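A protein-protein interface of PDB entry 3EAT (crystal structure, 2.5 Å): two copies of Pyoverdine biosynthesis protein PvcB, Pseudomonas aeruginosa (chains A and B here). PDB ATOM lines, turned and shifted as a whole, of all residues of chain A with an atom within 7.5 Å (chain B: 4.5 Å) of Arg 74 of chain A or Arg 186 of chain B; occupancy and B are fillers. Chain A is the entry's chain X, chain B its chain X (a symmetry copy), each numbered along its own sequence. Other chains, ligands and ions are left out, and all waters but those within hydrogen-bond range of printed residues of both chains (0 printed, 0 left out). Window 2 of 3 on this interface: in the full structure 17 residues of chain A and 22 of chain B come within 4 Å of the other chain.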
ATOM      1  N   PHE A  66       7.490  32.358  19.487  1.00  0.00           N
ATOM      2  CA  PHE A  66       6.796  31.357  20.304  1.00  0.00           C
ATOM      3  C   PHE A  66       6.633  31.935  21.709  1.00  0.00           C
ATOM      4  O   PHE A  66       7.593  32.442  22.288  1.00  0.00           O
ATOM      5  CB  PHE A  66       7.562  30.033  20.369  1.00  0.00           C
ATOM      6  CG  PHE A  66       7.738  29.384  19.035  1.00  0.00           C
ATOM      7  CD1 PHE A  66       6.702  28.654  18.466  1.00  0.00           C
ATOM      8  CD2 PHE A  66       8.927  29.533  18.332  1.00  0.00           C
ATOM      9  CE1 PHE A  66       6.843  28.081  17.210  1.00  0.00           C
ATOM     10  CE2 PHE A  66       9.091  28.941  17.076  1.00  0.00           C
ATOM     11  CZ  PHE A  66       8.049  28.208  16.511  1.00  0.00           C
ATOM     12  N   ALA A  67       5.420  31.873  22.248  1.00  0.00           N
ATOM     13  CA  ALA A  67       5.141  32.481  23.555  1.00  0.00           C
ATOM     14  C   ALA A  67       5.913  31.821  24.694  1.00  0.00           C
ATOM     15  O   ALA A  67       6.282  32.490  25.656  1.00  0.00           O
ATOM     16  CB  ALA A  67       3.646  32.486  23.847  1.00  0.00           C
ATOM     17  N   ASP A  68       6.168  30.522  24.579  1.00  0.00           N
ATOM     18  CA  ASP A  68       6.878  29.798  25.630  1.00  0.00           C
ATOM     19  C   ASP A  68       7.499  28.517  25.106  1.00  0.00           C
ATOM     20  O   ASP A  68       7.431  28.244  23.905  1.00  0.00           O
ATOM     21  CB  ASP A  68       5.938  29.492  26.809  1.00  0.00           C
ATOM     22  CG  ASP A  68       4.576  28.973  26.365  1.00  0.00           C
ATOM     23  OD1 ASP A  68       4.491  28.124  25.450  1.00  0.00           O
ATOM     24  OD2 ASP A  68       3.572  29.416  26.949  1.00  0.00           O
ATOM     25  N   ALA A  69       8.089  27.733  26.015  1.00  0.00           N
ATOM     26  CA  ALA A  69       8.770  26.485  25.662  1.00  0.00           C
ATOM     27  C   ALA A  69       7.813  25.404  25.160  1.00  0.00           C
ATOM     28  O   ALA A  69       8.156  24.636  24.250  1.00  0.00           O
ATOM     29  CB  ALA A  69       9.578  25.974  26.830  1.00  0.00           C
ATOM     30  N   GLU A  70       6.624  25.344  25.762  1.00  0.00           N
ATOM     31  CA  GLU A  70       5.585  24.391  25.371  1.00  0.00           C
ATOM     32  C   GLU A  70       5.172  24.635  23.907  1.00  0.00           C
ATOM     33  O   GLU A  70       5.014  23.690  23.135  1.00  0.00           O
ATOM     34  CB  GLU A  70       4.360  24.498  26.302  1.00  0.00           C
ATOM     35  CG  GLU A  70       4.607  24.146  27.787  1.00  0.00           C
ATOM     36  CD  GLU A  70       5.382  25.229  28.580  1.00  0.00           C
ATOM     37  OE1 GLU A  70       5.301  26.433  28.236  1.00  0.00           O
ATOM     38  OE2 GLU A  70       6.081  24.873  29.558  1.00  0.00           O
ATOM     39  N   SER A  71       5.016  25.908  23.540  1.00  0.00           N
ATOM     40  CA  SER A  71       4.659  26.300  22.184  1.00  0.00           C
ATOM     41  C   SER A  71       5.751  25.900  21.190  1.00  0.00           C
ATOM     42  O   SER A  71       5.468  25.324  20.131  1.00  0.00           O
ATOM     43  CB  SER A  71       4.420  27.799  22.110  1.00  0.00           C
ATOM     44  OG  SER A  71       4.031  28.152  20.801  1.00  0.00           O
ATOM     45  N   LEU A  72       7.000  26.184  21.551  1.00  0.00           N
ATOM     46  CA  LEU A  72       8.122  25.752  20.737  1.00  0.00           C
ATOM     47  C   LEU A  72       8.110  24.240  20.569  1.00  0.00           C
ATOM     48  O   LEU A  72       8.253  23.743  19.454  1.00  0.00           O
ATOM     49  CB  LEU A  72       9.449  26.244  21.323  1.00  0.00           C
ATOM     50  CG  LEU A  72      10.743  25.820  20.633  1.00  0.00           C
ATOM     51  CD1 LEU A  72      10.787  26.307  19.182  1.00  0.00           C
ATOM     52  CD2 LEU A  72      11.915  26.365  21.418  1.00  0.00           C
ATOM     53  N   THR A  73       7.926  23.516  21.668  1.00  0.00           N
ATOM     54  CA  THR A  73       7.860  22.046  21.651  1.00  0.00           C
ATOM     55  C   THR A  73       6.813  21.524  20.671  1.00  0.00           C
ATOM     56  O   THR A  73       7.087  20.630  19.873  1.00  0.00           O
ATOM     57  CB  THR A  73       7.569  21.486  23.059  1.00  0.00           C
ATOM     58  OG1 THR A  73       8.596  21.924  23.958  1.00  0.00           O
ATOM     59  CG2 THR A  73       7.546  19.963  23.040  1.00  0.00           C
ATOM     60  N   ARG A  74       5.613  22.085  20.716  1.00  0.00           N
ATOM     61  CA  ARG A  74       4.564  21.586  19.842  1.00  0.00           C
ATOM     62  C   ARG A  74       4.949  21.834  18.381  1.00  0.00           C
ATOM     63  O   ARG A  74       4.803  20.946  17.523  1.00  0.00           O
ATOM     64  CB  ARG A  74       3.217  22.204  20.189  1.00  0.00           C
ATOM     65  CG  ARG A  74       2.599  21.666  21.493  1.00  0.00           C
ATOM     66  CD  ARG A  74       1.162  22.155  21.687  1.00  0.00           C
ATOM     67  NE  ARG A  74       1.069  23.620  21.723  1.00  0.00           N
ATOM     68  CZ  ARG A  74       1.154  24.366  22.829  1.00  0.00           C
ATOM     69  NH1 ARG A  74       1.335  23.795  24.013  1.00  0.00           N
ATOM     70  NH2 ARG A  74       1.060  25.695  22.754  1.00  0.00           N
ATOM     71  N   TYR A  75       5.481  23.024  18.114  1.00  0.00           N
ATOM     72  CA  TYR A  75       5.967  23.352  16.788  1.00  0.00           C
ATOM     73  C   TYR A  75       6.976  22.314  16.317  1.00  0.00           C
ATOM     74  O   TYR A  75       6.856  21.792  15.212  1.00  0.00           O
ATOM     75  CB  TYR A  75       6.590  24.765  16.733  1.00  0.00           C
ATOM     76  CG  TYR A  75       7.276  25.029  15.407  1.00  0.00           C
ATOM     77  CD1 TYR A  75       6.540  25.454  14.301  1.00  0.00           C
ATOM     78  CD2 TYR A  75       8.645  24.806  15.243  1.00  0.00           C
ATOM     79  CE1 TYR A  75       7.151  25.674  13.080  1.00  0.00           C
ATOM     80  CE2 TYR A  75       9.263  25.013  14.012  1.00  0.00           C
ATOM     81  CZ  TYR A  75       8.506  25.457  12.937  1.00  0.00           C
ATOM     82  OH  TYR A  75       9.091  25.676  11.696  1.00  0.00           O
ATOM     83  N   CYS A  76       7.967  22.011  17.143  1.00  0.00           N
ATOM     84  CA  CYS A  76       9.003  21.044  16.735  1.00  0.00           C
ATOM     85  C   CYS A  76       8.468  19.643  16.475  1.00  0.00           C
ATOM     86  O   CYS A  76       8.981  18.931  15.589  1.00  0.00           O
ATOM     87  CB  CYS A  76      10.159  20.998  17.725  1.00  0.00           C
ATOM     88  SG  CYS A  76      11.115  22.535  17.778  1.00  0.00           S
ATOM     89  N   HIS A  77       7.436  19.253  17.235  1.00  0.00           N
ATOM     90  CA  HIS A  77       6.791  17.948  17.039  1.00  0.00           C
ATOM     91  C   HIS A  77       6.187  17.845  15.640  1.00  0.00           C
ATOM     92  O   HIS A  77       6.214  16.774  15.036  1.00  0.00           O
ATOM     93  CB  HIS A  77       5.763  17.631  18.141  1.00  0.00           C
ATOM     94  CG  HIS A  77       6.386  17.129  19.411  1.00  0.00           C
ATOM     95  ND1 HIS A  77       7.276  16.072  19.435  1.00  0.00           N
ATOM     96  CD2 HIS A  77       6.263  17.545  20.696  1.00  0.00           C
ATOM     97  CE1 HIS A  77       7.678  15.864  20.679  1.00  0.00           C
ATOM     98  NE2 HIS A  77       7.083  16.747  21.461  1.00  0.00           N
ATOM     99  N   ASP A  78       5.683  18.968  15.130  1.00  0.00           N
ATOM    100  CA  ASP A  78       5.160  19.049  13.769  1.00  0.00           C
ATOM    101  C   ASP A  78       6.290  19.111  12.733  1.00  0.00           C
ATOM    102  O   ASP A  78       6.155  18.622  11.623  1.00  0.00           O
ATOM    103  CB  ASP A  78       4.258  20.271  13.616  1.00  0.00           C
ATOM    104  CG  ASP A  78       3.475  20.253  12.316  1.00  0.00           C
ATOM    105  OD1 ASP A  78       2.734  19.276  12.089  1.00  0.00           O
ATOM    106  OD2 ASP A  78       3.587  21.211  11.512  1.00  0.00           O
ATOM    107  N   PHE A  79       7.397  19.722  13.119  1.00  0.00           N
ATOM    108  CA  PHE A  79       8.539  19.921  12.253  1.00  0.00           C
ATOM    109  C   PHE A  79       9.200  18.589  11.857  1.00  0.00           C
ATOM    110  O   PHE A  79       9.518  18.376  10.692  1.00  0.00           O
ATOM    111  CB  PHE A  79       9.525  20.842  12.986  1.00  0.00           C
ATOM    112  CG  PHE A  79      10.748  21.187  12.204  1.00  0.00           C
ATOM    113  CD1 PHE A  79      10.814  22.376  11.480  1.00  0.00           C
ATOM    114  CD2 PHE A  79      11.849  20.344  12.208  1.00  0.00           C
ATOM    115  CE1 PHE A  79      11.961  22.716  10.767  1.00  0.00           C
ATOM    116  CE2 PHE A  79      13.007  20.669  11.485  1.00  0.00           C
ATOM    117  CZ  PHE A  79      13.061  21.855  10.765  1.00  0.00           C
ATOM    118  N   GLY A  80       9.403  17.693  12.820  1.00  0.00           N
ATOM    119  CA  GLY A  80      10.064  16.397  12.564  1.00  0.00           C
ATOM    120  C   GLY A  80       9.940  15.547  13.803  1.00  0.00           C
ATOM    121  O   GLY A  80       9.126  15.862  14.671  1.00  0.00           O
ATOM    122  N   VAL A  82      11.177  14.956  17.264  1.00  0.00           N
ATOM    123  CA  VAL A  82      11.999  15.551  18.305  1.00  0.00           C
ATOM    124  C   VAL A  82      12.832  14.428  18.918  1.00  0.00           C
ATOM    125  O   VAL A  82      12.325  13.335  19.126  1.00  0.00           O
ATOM    126  CB  VAL A  82      11.111  16.244  19.362  1.00  0.00           C
ATOM    127  CG1 VAL A  82      11.927  16.745  20.529  1.00  0.00           C
ATOM    128  CG2 VAL A  82      10.309  17.378  18.731  1.00  0.00           C
ATOM    129  N   ALA A  89      11.968  18.084  25.564  1.00  0.00           N
ATOM    130  CA  ALA A  89      12.316  18.549  24.222  1.00  0.00           C
ATOM    131  C   ALA A  89      13.272  19.738  24.239  1.00  0.00           C
ATOM    132  O   ALA A  89      14.185  19.813  23.404  1.00  0.00           O
ATOM    133  CB  ALA A  89      11.044  18.905  23.436  1.00  0.00           C
ATOM    134  N   VAL A  90      13.061  20.651  25.191  1.00  0.00           N
ATOM    135  CA  VAL A  90      13.741  21.951  25.216  1.00  0.00           C
ATOM    136  C   VAL A  90      14.838  22.088  26.288  1.00  0.00           C
ATOM    137  O   VAL A  90      14.560  22.028  27.486  1.00  0.00           O
ATOM    138  CB  VAL A  90      12.725  23.089  25.397  1.00  0.00           C
ATOM    139  CG1 VAL A  90      13.430  24.435  25.494  1.00  0.00           C
ATOM    140  CG2 VAL A  90      11.725  23.095  24.262  1.00  0.00           C
ATOM    141  N   GLU B 185      -7.364  31.603  18.761  1.00  0.00           N
ATOM    142  CA  GLU B 185      -6.864  30.260  18.931  1.00  0.00           C
ATOM    143  C   GLU B 185      -5.397  30.220  18.445  1.00  0.00           C
ATOM    144  O   GLU B 185      -4.870  31.223  17.931  1.00  0.00           O
ATOM    145  CB  GLU B 185      -7.814  29.328  18.168  1.00  0.00           C
ATOM    146  CG  GLU B 185      -7.526  27.859  18.219  1.00  0.00           C
ATOM    147  CD  GLU B 185      -7.612  27.257  19.603  1.00  0.00           C
ATOM    148  OE1 GLU B 185      -8.720  26.807  19.990  1.00  0.00           O
ATOM    149  OE2 GLU B 185      -6.556  27.192  20.277  1.00  0.00           O
ATOM    150  N   ARG B 186      -4.724  29.099  18.667  1.00  0.00           N
ATOM    151  CA  ARG B 186      -3.446  28.835  18.043  1.00  0.00           C
ATOM    152  C   ARG B 186      -3.652  27.806  16.917  1.00  0.00           C
ATOM    153  O   ARG B 186      -4.510  26.920  17.027  1.00  0.00           O
ATOM    154  CB  ARG B 186      -2.431  28.336  19.073  1.00  0.00           C
ATOM    155  CG  ARG B 186      -2.797  27.018  19.725  1.00  0.00           C
ATOM    156  CD  ARG B 186      -1.625  26.460  20.478  1.00  0.00           C
ATOM    157  NE  ARG B 186      -1.915  25.163  21.095  1.00  0.00           N
ATOM    158  CZ  ARG B 186      -2.164  24.982  22.397  1.00  0.00           C
ATOM    159  NH1 ARG B 186      -2.180  26.017  23.235  1.00  0.00           N
ATOM    160  NH2 ARG B 186      -2.392  23.764  22.868  1.00  0.00           N
ATOM    161  N   HIS B 187      -2.886  27.918  15.836  1.00  0.00           N
ATOM    162  CA  HIS B 187      -2.983  26.937  14.777  1.00  0.00           C
ATOM    163  C   HIS B 187      -2.699  25.578  15.401  1.00  0.00           C
ATOM    164  O   HIS B 187      -1.726  25.427  16.118  1.00  0.00           O
ATOM    165  CB  HIS B 187      -2.002  27.250  13.645  1.00  0.00           C
ATOM    166  CG  HIS B 187      -2.116  26.325  12.483  1.00  0.00           C
ATOM    167  ND1 HIS B 187      -1.643  25.029  12.516  1.00  0.00           N
ATOM    168  CD2 HIS B 187      -2.648  26.504  11.249  1.00  0.00           C
ATOM    169  CE1 HIS B 187      -1.882  24.445  11.353  1.00  0.00           C
ATOM    170  NE2 HIS B 187      -2.488  25.321  10.564  1.00  0.00           N
ATOM    171  N   PRO B 188      -3.563  24.587  15.150  1.00  0.00           N
ATOM    172  CA  PRO B 188      -3.478  23.296  15.865  1.00  0.00           C
ATOM    173  C   PRO B 188      -2.245  22.443  15.547  1.00  0.00           C
ATOM    174  O   PRO B 188      -2.052  21.402  16.164  1.00  0.00           O
ATOM    175  CB  PRO B 188      -4.745  22.561  15.412  1.00  0.00           C
ATOM    176  CG  PRO B 188      -5.042  23.161  14.046  1.00  0.00           C
ATOM    177  CD  PRO B 188      -4.691  24.617  14.196  1.00  0.00           C
ATOM    178  N   ARG B 189      -1.425  22.862  14.597  1.00  0.00           N
ATOM    179  CA  ARG B 189      -0.208  22.115  14.264  1.00  0.00           C
ATOM    180  C   ARG B 189       1.040  22.989  14.273  1.00  0.00           C
ATOM    181  O   ARG B 189       2.109  22.510  14.655  1.00  0.00           O
ATOM    182  CB  ARG B 189      -0.331  21.418  12.900  1.00  0.00           C
ATOM    183  CG  ARG B 189      -1.246  20.204  12.873  1.00  0.00           C
ATOM    184  CD  ARG B 189      -0.618  18.994  13.585  1.00  0.00           C
ATOM    185  NE  ARG B 189      -1.205  17.741  13.107  1.00  0.00           N
ATOM    186  CZ  ARG B 189      -2.227  17.137  13.690  1.00  0.00           C
ATOM    187  NH1 ARG B 189      -2.771  17.670  14.766  1.00  0.00           N
ATOM    188  NH2 ARG B 189      -2.713  16.006  13.202  1.00  0.00           N
ATOM    189  N   GLU B 191       1.221  26.399  15.487  1.00  0.00           N
ATOM    190  CA  GLU B 191       1.283  27.323  16.630  1.00  0.00           C
ATOM    191  C   GLU B 191       0.873  28.754  16.410  1.00  0.00           C
ATOM    192  O   GLU B 191       0.441  29.410  17.361  1.00  0.00           O
ATOM    193  CB  GLU B 191       2.640  27.285  17.325  1.00  0.00           C
ATOM    194  CG  GLU B 191       2.867  25.988  18.068  1.00  0.00           C
ATOM    195  CD  GLU B 191       1.895  25.807  19.236  1.00  0.00           C
ATOM    196  OE1 GLU B 191       1.821  26.696  20.139  1.00  0.00           O
ATOM    197  OE2 GLU B 191       1.203  24.768  19.237  1.00  0.00           O
ATOM    198  N   PHE B 192       0.988  29.258  15.184  1.00  0.00           N
ATOM    199  CA  PHE B 192       0.776  30.689  14.995  1.00  0.00           C
ATOM    200  C   PHE B 192      -0.657  31.096  15.383  1.00  0.00           C
ATOM    201  O   PHE B 192      -1.553  30.253  15.385  1.00  0.00           O
ATOM    202  CB  PHE B 192       1.194  31.155  13.589  1.00  0.00           C
ATOM    203  CG  PHE B 192       0.458  30.491  12.464  1.00  0.00           C
ATOM    204  CD1 PHE B 192      -0.678  31.079  11.919  1.00  0.00           C
ATOM    205  CD2 PHE B 192       0.924  29.309  11.915  1.00  0.00           C
ATOM    206  CE1 PHE B 192      -1.369  30.469  10.856  1.00  0.00           C
ATOM    207  CE2 PHE B 192       0.246  28.700  10.846  1.00  0.00           C
ATOM    208  CZ  PHE B 192      -0.896  29.281  10.323  1.00  0.00           C
ATOM    209  N   ILE B 194      -4.387  32.290  15.238  1.00  0.00           N
ATOM    210  CA  ILE B 194      -5.464  32.278  14.260  1.00  0.00           C
ATOM    211  C   ILE B 194      -6.773  32.660  14.954  1.00  0.00           C
ATOM    212  O   ILE B 194      -6.820  32.796  16.182  1.00  0.00           O
ATOM    213  CB  ILE B 194      -5.606  30.884  13.591  1.00  0.00           C
ATOM    214  CG1 ILE B 194      -5.917  29.799  14.639  1.00  0.00           C
ATOM    215  CG2 ILE B 194      -4.346  30.533  12.768  1.00  0.00           C
ATOM    216  CD1 ILE B 194      -6.444  28.482  14.038  1.00  0.00           C
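Arg 74 of chain A touches just these residues of chain B: Arg 186 (3.3 Å) and Glu 191 (2.7 Å). Arg 186 of chain B touches one residue of chain A. Of the printed residues of chain B, Ser 71 of chain A touches Glu 191. Of the printed residues of chain B, Tyr 75 of chain A touches Glu 191 (3.95 Å). Printed residues of chain A within 4 Å of Glu 191 of chain B: Ser 71, Arg 74 and Tyr 75. Printed residues of chain B within 4 Å of Asp 78 of chain A: Arg 189. Printed residues of chain A within 4 Å of Arg 189 of chain B: Asp 78. Cys 76 of chain A touches none of the printed residues of chain B.
Of the 8 printed residues of chain B, 3 touch a printed residue of chain A. Printed residues of chain B that touch a printed residue of chain A: Arg 186, Arg 189 and Glu 191. Of the 18 printed residues of chain A, 4 touch a printed residue of chain B. Printed residues of chain A that touch a printed residue of chain B: Ser 71, Arg 74, Tyr 75 and Asp 78.
No position is printed for both chains.
The side-chain carboxylate (OE1) of Glu 191 of chain B is in hydrogen-bond range of the side-chain hydroxyl (OG) of Ser 71 of chain A (2.7 Å). The guanidinium group of Arg 74 of chain A is in salt-bridge range of the side-chain carboxylate of Glu 191 of chain B (2.7 Å). The guanidinium group of Arg 186 of chain B lies close to the guanidinium group of Arg 74 of chain A (3.3 Å).
Among the printed residues, merely in contact across the chains: Tyr 75 of chain A with Glu 191 of chain B and Asp 78 of chain A with Arg 189 of chain B.
N of Arg 189 of chain B is in hydrogen-bond range of ND1 of His 187 of chain B, at 3.0 Å. N of Ser 71 of chain A is in hydrogen-bond range of OD1 of Asp 68 of chain A. OE2 of Glu 191 of chain B lies within salt-bridge range of NE of Arg 186 of chain B, 3.7 Å away.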
